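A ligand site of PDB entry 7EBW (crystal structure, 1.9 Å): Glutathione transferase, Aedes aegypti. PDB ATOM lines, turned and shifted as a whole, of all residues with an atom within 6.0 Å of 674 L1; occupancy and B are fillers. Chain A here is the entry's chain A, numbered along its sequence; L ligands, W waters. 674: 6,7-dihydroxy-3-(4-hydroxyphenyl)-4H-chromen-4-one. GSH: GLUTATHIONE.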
ATOM      1  N   ILE A  18     -12.151  10.574  -8.790  1.00  0.00           N
ATOM      2  CA  ILE A  18     -11.605  11.894  -9.099  1.00  0.00           C
ATOM      3  C   ILE A  18     -10.284  12.155  -8.374  1.00  0.00           C
ATOM      4  O   ILE A  18      -9.474  12.964  -8.831  1.00  0.00           O
ATOM      5  CB  ILE A  18     -12.734  12.900  -8.826  1.00  0.00           C
ATOM      6  CG1 ILE A  18     -12.995  13.068  -7.326  1.00  0.00           C
ATOM      7  CG2 ILE A  18     -13.996  12.549  -9.620  1.00  0.00           C
ATOM      8  CD1 ILE A  18     -13.320  14.457  -6.952  1.00  0.00           C
ATOM      9  N   SER A  19     -10.035  11.424  -7.280  1.00  0.00           N
ATOM     10  CA  SER A  19      -8.833  11.560  -6.461  1.00  0.00           C
ATOM     11  C   SER A  19      -7.650  10.858  -7.121  1.00  0.00           C
ATOM     12  O   SER A  19      -7.744   9.656  -7.399  1.00  0.00           O
ATOM     13  CB  SER A  19      -9.096  10.963  -5.082  1.00  0.00           C
ATOM     14  OG  SER A  19      -7.906  10.695  -4.367  1.00  0.00           O
ATOM     15  N   PRO A  20      -6.528  11.546  -7.391  1.00  0.00           N
ATOM     16  CA  PRO A  20      -5.326  10.860  -7.907  1.00  0.00           C
ATOM     17  C   PRO A  20      -4.862   9.729  -6.995  1.00  0.00           C
ATOM     18  O   PRO A  20      -4.575   8.625  -7.487  1.00  0.00           O
ATOM     19  CB  PRO A  20      -4.276  11.987  -7.968  1.00  0.00           C
ATOM     20  CG  PRO A  20      -5.050  13.227  -8.036  1.00  0.00           C
ATOM     21  CD  PRO A  20      -6.327  12.991  -7.263  1.00  0.00           C
ATOM     22  N   PRO A  21      -4.771   9.926  -5.664  1.00  0.00           N
ATOM     23  CA  PRO A  21      -4.408   8.785  -4.807  1.00  0.00           C
ATOM     24  C   PRO A  21      -5.295   7.570  -5.013  1.00  0.00           C
ATOM     25  O   PRO A  21      -4.793   6.433  -5.063  1.00  0.00           O
ATOM     26  CB  PRO A  21      -4.557   9.352  -3.381  1.00  0.00           C
ATOM     27  CG  PRO A  21      -4.266  10.773  -3.530  1.00  0.00           C
ATOM     28  CD  PRO A  21      -4.864  11.160  -4.865  1.00  0.00           C
ATOM     29  N   ARG A  23      -6.851   6.834  -7.803  1.00  0.00           N
ATOM     30  CA  ARG A  23      -6.583   6.267  -9.124  1.00  0.00           C
ATOM     31  C   ARG A  23      -5.242   5.540  -9.157  1.00  0.00           C
ATOM     32  O   ARG A  23      -5.076   4.590  -9.937  1.00  0.00           O
ATOM     33  CB  ARG A  23      -6.642   7.367 -10.185  1.00  0.00           C
ATOM     34  CG  ARG A  23      -8.069   7.745 -10.559  1.00  0.00           C
ATOM     35  CD  ARG A  23      -8.117   8.841 -11.600  1.00  0.00           C
ATOM     36  NE  ARG A  23      -8.128  10.175 -11.002  1.00  0.00           N
ATOM     37  CZ  ARG A  23      -7.124  11.037 -11.098  1.00  0.00           C
ATOM     38  NH1 ARG A  23      -5.988  10.725 -11.714  1.00  0.00           N
ATOM     39  NH2 ARG A  23      -7.271  12.258 -10.584  1.00  0.00           N
ATOM     40  N   LEU A  45     -16.680  12.593  -2.688  1.00  0.00           N
ATOM     41  CA  LEU A  45     -16.114  13.765  -2.024  1.00  0.00           C
ATOM     42  C   LEU A  45     -17.009  14.984  -2.176  1.00  0.00           C
ATOM     43  O   LEU A  45     -17.243  15.714  -1.212  1.00  0.00           O
ATOM     44  CB  LEU A  45     -14.721  14.047  -2.587  1.00  0.00           C
ATOM     45  CG  LEU A  45     -13.699  12.956  -2.231  1.00  0.00           C
ATOM     46  CD1 LEU A  45     -12.344  13.219  -2.914  1.00  0.00           C
ATOM     47  CD2 LEU A  45     -13.560  12.952  -0.739  1.00  0.00           C
ATOM     48  N   PHE A  46     -17.487  15.255  -3.396  1.00  0.00           N
ATOM     49  CA  PHE A  46     -18.323  16.428  -3.585  1.00  0.00           C
ATOM     50  C   PHE A  46     -19.685  16.279  -2.928  1.00  0.00           C
ATOM     51  O   PHE A  46     -20.378  17.277  -2.714  1.00  0.00           O
ATOM     52  CB  PHE A  46     -18.468  16.750  -5.075  1.00  0.00           C
ATOM     53  CG  PHE A  46     -17.319  17.544  -5.628  1.00  0.00           C
ATOM     54  CD1 PHE A  46     -17.188  18.899  -5.351  1.00  0.00           C
ATOM     55  CD2 PHE A  46     -16.329  16.928  -6.373  1.00  0.00           C
ATOM     56  CE1 PHE A  46     -16.129  19.624  -5.830  1.00  0.00           C
ATOM     57  CE2 PHE A  46     -15.263  17.654  -6.860  1.00  0.00           C
ATOM     58  CZ  PHE A  46     -15.153  18.997  -6.588  1.00  0.00           C
ATOM     59  N   ARG A  48     -19.737  15.025   0.109  1.00  0.00           N
ATOM     60  CA  ARG A  48     -19.264  15.112   1.491  1.00  0.00           C
ATOM     61  C   ARG A  48     -19.550  13.819   2.271  1.00  0.00           C
ATOM     62  O   ARG A  48     -19.643  13.828   3.497  1.00  0.00           O
ATOM     63  CB  ARG A  48     -19.833  16.348   2.203  1.00  0.00           C
ATOM     64  CG  ARG A  48     -19.399  17.653   1.499  1.00  0.00           C
ATOM     65  CD  ARG A  48     -19.709  18.899   2.311  1.00  0.00           C
ATOM     66  NE  ARG A  48     -21.147  19.003   2.538  1.00  0.00           N
ATOM     67  CZ  ARG A  48     -21.988  19.686   1.781  1.00  0.00           C
ATOM     68  NH1 ARG A  48     -21.573  20.399   0.752  1.00  0.00           N
ATOM     69  NH2 ARG A  48     -23.287  19.656   2.071  1.00  0.00           N
ATOM     70  N   HIS A  50     -17.367  11.677   2.779  1.00  0.00           N
ATOM     71  CA  HIS A  50     -16.185  11.418   3.604  1.00  0.00           C
ATOM     72  C   HIS A  50     -16.274  12.076   4.961  1.00  0.00           C
ATOM     73  O   HIS A  50     -15.411  11.834   5.810  1.00  0.00           O
ATOM     74  CB  HIS A  50     -14.922  11.891   2.879  1.00  0.00           C
ATOM     75  CG  HIS A  50     -14.928  13.358   2.558  1.00  0.00           C
ATOM     76  ND1 HIS A  50     -15.869  13.923   1.720  1.00  0.00           N
ATOM     77  CD2 HIS A  50     -14.102  14.361   2.928  1.00  0.00           C
ATOM     78  CE1 HIS A  50     -15.643  15.229   1.619  1.00  0.00           C
ATOM     79  NE2 HIS A  50     -14.576  15.514   2.342  1.00  0.00           N
ATOM     80  N   LEU A  51     -17.288  12.911   5.198  1.00  0.00           N
ATOM     81  CA  LEU A  51     -17.466  13.562   6.486  1.00  0.00           C
ATOM     82  C   LEU A  51     -18.518  12.878   7.332  1.00  0.00           C
ATOM     83  O   LEU A  51     -18.766  13.313   8.460  1.00  0.00           O
ATOM     84  CB  LEU A  51     -17.824  15.041   6.276  1.00  0.00           C
ATOM     85  CG  LEU A  51     -16.779  15.804   5.448  1.00  0.00           C
ATOM     86  CD1 LEU A  51     -17.171  17.282   5.200  1.00  0.00           C
ATOM     87  CD2 LEU A  51     -15.445  15.741   6.151  1.00  0.00           C
ATOM     88  N   PHE A 117       2.395  14.735  -5.195  1.00  0.00           N
ATOM     89  CA  PHE A 117       0.995  14.881  -4.819  1.00  0.00           C
ATOM     90  C   PHE A 117       0.809  16.035  -3.848  1.00  0.00           C
ATOM     91  O   PHE A 117      -0.212  16.729  -3.903  1.00  0.00           O
ATOM     92  CB  PHE A 117       0.426  13.593  -4.218  1.00  0.00           C
ATOM     93  CG  PHE A 117      -0.945  13.796  -3.621  1.00  0.00           C
ATOM     94  CD1 PHE A 117      -2.035  14.017  -4.457  1.00  0.00           C
ATOM     95  CD2 PHE A 117      -1.136  13.809  -2.241  1.00  0.00           C
ATOM     96  CE1 PHE A 117      -3.286  14.228  -3.943  1.00  0.00           C
ATOM     97  CE2 PHE A 117      -2.403  14.017  -1.729  1.00  0.00           C
ATOM     98  CZ  PHE A 117      -3.485  14.232  -2.584  1.00  0.00           C
ATOM     99  N   GLU A 120       0.683  19.019  -6.096  1.00  0.00           N
ATOM    100  CA  GLU A 120      -0.552  18.993  -6.861  1.00  0.00           C
ATOM    101  C   GLU A 120      -1.739  19.374  -5.996  1.00  0.00           C
ATOM    102  O   GLU A 120      -2.626  20.137  -6.434  1.00  0.00           O
ATOM    103  CB  GLU A 120      -0.759  17.611  -7.494  1.00  0.00           C
ATOM    104  CG  GLU A 120      -2.033  17.436  -8.361  1.00  0.00           C
ATOM    105  CD  GLU A 120      -3.315  17.096  -7.619  1.00  0.00           C
ATOM    106  OE1 GLU A 120      -3.278  16.639  -6.460  1.00  0.00           O
ATOM    107  OE2 GLU A 120      -4.374  17.281  -8.219  1.00  0.00           O
ATOM    108  N   SER A 121      -1.780  18.880  -4.763  1.00  0.00           N
ATOM    109  CA  SER A 121      -2.973  19.055  -3.943  1.00  0.00           C
ATOM    110  C   SER A 121      -3.112  20.474  -3.419  1.00  0.00           C
ATOM    111  O   SER A 121      -4.235  20.971  -3.276  1.00  0.00           O
ATOM    112  CB  SER A 121      -2.979  18.067  -2.777  1.00  0.00           C
ATOM    113  OG  SER A 121      -1.871  18.299  -1.940  1.00  0.00           O
ATOM    114  N   ILE A 122      -1.999  21.155  -3.114  1.00  0.00           N
ATOM    115  CA  ILE A 122      -2.100  22.571  -2.740  1.00  0.00           C
ATOM    116  C   ILE A 122      -2.802  23.369  -3.830  1.00  0.00           C
ATOM    117  O   ILE A 122      -3.688  24.182  -3.549  1.00  0.00           O
ATOM    118  CB  ILE A 122      -0.700  23.155  -2.417  1.00  0.00           C
ATOM    119  CG1 ILE A 122      -0.222  22.692  -1.058  1.00  0.00           C
ATOM    120  CG2 ILE A 122      -0.682  24.684  -2.545  1.00  0.00           C
ATOM    121  CD1 ILE A 122       1.275  22.539  -0.954  1.00  0.00           C
ATOM    122  N   MET A 124      -4.678  22.131  -6.531  1.00  0.00           N
ATOM    123  CA  MET A 124      -6.002  21.600  -6.814  1.00  0.00           C
ATOM    124  C   MET A 124      -7.004  21.920  -5.713  1.00  0.00           C
ATOM    125  O   MET A 124      -8.142  22.313  -6.002  1.00  0.00           O
ATOM    126  CB  MET A 124      -5.922  20.089  -7.077  1.00  0.00           C
ATOM    127  CG  MET A 124      -6.927  19.621  -8.096  1.00  0.00           C
ATOM    128  SD  MET A 124      -6.861  20.413  -9.726  1.00  0.00           S
ATOM    129  CE  MET A 124      -5.129  20.354 -10.126  1.00  0.00           C
ATOM    130  N   ARG A 125      -6.616  21.775  -4.442  1.00  0.00           N
ATOM    131  CA  ARG A 125      -7.524  22.101  -3.344  1.00  0.00           C
ATOM    132  C   ARG A 125      -7.875  23.581  -3.344  1.00  0.00           C
ATOM    133  O   ARG A 125      -9.025  23.965  -3.123  1.00  0.00           O
ATOM    134  CB  ARG A 125      -6.885  21.716  -2.002  1.00  0.00           C
ATOM    135  CG  ARG A 125      -7.219  20.325  -1.488  1.00  0.00           C
ATOM    136  CD  ARG A 125      -6.333  19.954  -0.285  1.00  0.00           C
ATOM    137  NE  ARG A 125      -6.736  20.555   0.975  1.00  0.00           N
ATOM    138  CZ  ARG A 125      -7.637  20.049   1.811  1.00  0.00           C
ATOM    139  NH1 ARG A 125      -8.299  18.932   1.513  1.00  0.00           N
ATOM    140  NH2 ARG A 125      -7.869  20.648   2.961  1.00  0.00           N
ATOM    141  N   ILE A 128     -10.369  24.164  -6.229  1.00  0.00           N
ATOM    142  CA  ILE A 128     -11.694  23.591  -5.971  1.00  0.00           C
ATOM    143  C   ILE A 128     -12.459  24.439  -4.956  1.00  0.00           C
ATOM    144  O   ILE A 128     -13.634  24.762  -5.144  1.00  0.00           O
ATOM    145  CB  ILE A 128     -11.583  22.130  -5.518  1.00  0.00           C
ATOM    146  CG1 ILE A 128     -11.183  21.227  -6.683  1.00  0.00           C
ATOM    147  CG2 ILE A 128     -12.885  21.660  -4.885  1.00  0.00           C
ATOM    148  CD1 ILE A 128     -10.834  19.795  -6.270  1.00  0.00           C
ATOM    149  N   THR A 178      -3.272  14.554 -13.558  1.00  0.00           N
ATOM    150  CA  THR A 178      -4.151  15.517 -12.907  1.00  0.00           C
ATOM    151  C   THR A 178      -3.535  16.912 -12.923  1.00  0.00           C
ATOM    152  O   THR A 178      -4.157  17.855 -13.411  1.00  0.00           O
ATOM    153  CB  THR A 178      -4.428  15.101 -11.463  1.00  0.00           C
ATOM    154  OG1 THR A 178      -4.826  13.740 -11.452  1.00  0.00           O
ATOM    155  CG2 THR A 178      -5.516  15.959 -10.887  1.00  0.00           C
ATOM    156  N   LEU A 217     -12.895  15.080 -12.991  1.00  0.00           N
ATOM    157  CA  LEU A 217     -12.287  16.219 -12.300  1.00  0.00           C
ATOM    158  C   LEU A 217     -12.141  17.404 -13.242  1.00  0.00           C
ATOM    159  O   LEU A 217     -12.392  18.556 -12.830  1.00  0.00           O
ATOM    160  CB  LEU A 217     -10.931  15.817 -11.717  1.00  0.00           C
ATOM    161  CG  LEU A 217     -10.186  16.867 -10.906  1.00  0.00           C
ATOM    162  CD1 LEU A 217     -11.021  17.355  -9.741  1.00  0.00           C
ATOM    163  CD2 LEU A 217      -8.917  16.256 -10.381  1.00  0.00           C
HETATM  164  C8A 674 L   1      -9.525  16.430  -5.628  1.00  0.00           C
HETATM  165  C4A 674 L   1      -9.118  17.140  -4.478  1.00  0.00           C
HETATM  166  C4  674 L   1     -10.094  17.521  -3.450  1.00  0.00           C
HETATM  167  C3  674 L   1     -11.464  17.171  -3.640  1.00  0.00           C
HETATM  168  C2  674 L   1     -11.886  16.435  -4.844  1.00  0.00           C
HETATM  169  O1  674 L   1     -10.952  16.036  -5.895  1.00  0.00           O
HETATM  170  C8  674 L   1      -8.626  16.040  -6.615  1.00  0.00           C
HETATM  171  C7  674 L   1      -7.286  16.375  -6.463  1.00  0.00           C
HETATM  172  C6  674 L   1      -6.836  17.073  -5.306  1.00  0.00           C
HETATM  173  C5  674 L   1      -7.748  17.467  -4.316  1.00  0.00           C
HETATM  174  O4  674 L   1      -6.437  15.980  -7.490  1.00  0.00           O
HETATM  175  O3  674 L   1      -5.487  17.388  -5.149  1.00  0.00           O
HETATM  176  C1' 674 L   1     -12.593  17.510  -2.673  1.00  0.00           C
HETATM  177  C2' 674 L   1     -13.809  17.959  -3.193  1.00  0.00           C
HETATM  178  C3' 674 L   1     -14.852  18.277  -2.339  1.00  0.00           C
HETATM  179  C4' 674 L   1     -14.690  18.092  -0.969  1.00  0.00           C
HETATM  180  C5' 674 L   1     -13.496  17.609  -0.458  1.00  0.00           C
HETATM  181  C6' 674 L   1     -12.449  17.321  -1.304  1.00  0.00           C
HETATM  182  O5  674 L   1     -15.742  18.394  -0.099  1.00  0.00           O
HETATM  183  O2  674 L   1      -9.748  18.118  -2.477  1.00  0.00           O
HETATM  184  N1  GSH L   2      -1.648  10.793   1.199  1.00  0.00           N
HETATM  185  CA1 GSH L   2      -3.069  10.382   1.011  1.00  0.00           C
HETATM  186  C1  GSH L   2      -3.143   9.157   0.084  1.00  0.00           C
HETATM  187  O11 GSH L   2      -2.260   9.057  -0.786  1.00  0.00           O
HETATM  188  O12 GSH L   2      -4.091   8.346   0.268  1.00  0.00           O
HETATM  189  CB1 GSH L   2      -3.877  11.564   0.464  1.00  0.00           C
HETATM  190  CG1 GSH L   2      -5.380  11.311   0.375  1.00  0.00           C
HETATM  191  CD1 GSH L   2      -6.090  12.584  -0.034  1.00  0.00           C
HETATM  192  OE1 GSH L   2      -5.566  13.689   0.106  1.00  0.00           O
HETATM  193  N2  GSH L   2      -7.315  12.430  -0.555  1.00  0.00           N
HETATM  194  CA2 GSH L   2      -8.191  13.540  -0.847  1.00  0.00           C
HETATM  195  C2  GSH L   2      -9.419  13.645   0.050  1.00  0.00           C
HETATM  196  O2  GSH L   2     -10.094  12.634   0.252  1.00  0.00           O
HETATM  197  CB2 GSH L   2      -8.646  13.491  -2.298  1.00  0.00           C
HETATM  198  SG2 GSH L   2      -7.297  13.760  -3.469  1.00  0.00           S
HETATM  199  N3  GSH L   2      -9.691  14.839   0.566  1.00  0.00           N
HETATM  200  CA3 GSH L   2     -10.828  15.072   1.436  1.00  0.00           C
HETATM  201  C3  GSH L   2     -10.425  15.856   2.683  1.00  0.00           C
HETATM  202  O31 GSH L   2      -9.210  16.119   2.805  1.00  0.00           O
HETATM  203  O32 GSH L   2     -11.325  16.189   3.471  1.00  0.00           O
HETATM  204  O   HOH W   1     -17.701  19.560  -1.219  1.00  0.00           O
HETATM  205  O   HOH W   2      -8.130  17.108  -0.429  1.00  0.00           O
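The side-chain carboxylate (OE2) of Glu 120 is in hydrogen-bond range of an oxygen (O4) of 674 L1, at 2.5 Å.
O5 of 674 L1 lies within hydrogen-bond range of O of Leu 45 (3.3 Å).
NH1 of Arg 125 is in salt-bridge range of O31 of GSH L2 (3.2 Å).
OG of Ser 19 sits close to SG2 of GSH L2.
O of Ile 18 is in hydrogen-bond range of NH2 of Arg 23, at 2.9 Å.
The backbone carbonyl oxygen (O) of Phe 117 is in hydrogen-bond range of the side-chain hydroxyl (OG) of Ser 121 (3.0 Å).
The side-chain hydroxyl (OG1) of Thr 178 is in hydrogen-bond range of the guanidinium group (NH2) of Arg 23 (3.0 Å).
Water W2 lies within hydrogen-bond range of the guanidinium group of Arg 125 (2.7 Å), an oxygen (O2) of 674 L1 (2.8 Å) and a nitrogen (N3) of GSH L2 (2.9 Å).
Ile 18 touches 674 L1 (CD1 to O1, 3.0 Å).
CD of Pro 20 touches O4 of 674 L1 (3.0 Å).
Phe 46 touches 674 L1.
His 50 touches 674 L1.
Ser 121 touches 674 L1 (CA to O3, 3.2 Å).
CB of Met 124 touches O3 of 674 L1 (3.3 Å).
CG of Arg 125 touches O2 of 674 L1, 3.5 Å away.
CD1 of Ile 128 touches C4A of 674 L1, 3.6 Å away.
Thr 178 touches 674 L1 (CG2 to O4, 3.5 Å).
Leu 217 touches 674 L1 (CD2 to C8, 3.8 Å).
Within 4 Å of 674 L1: Ile 18, Pro 20, Leu 45, Phe 46, His 50, Glu 120, Ser 121, Met 124, Arg 125, Ile 128, Thr 178 and Leu 217.
The nearest printed residue that does not touch 674 L1 is Phe 117 (4.04 Å).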
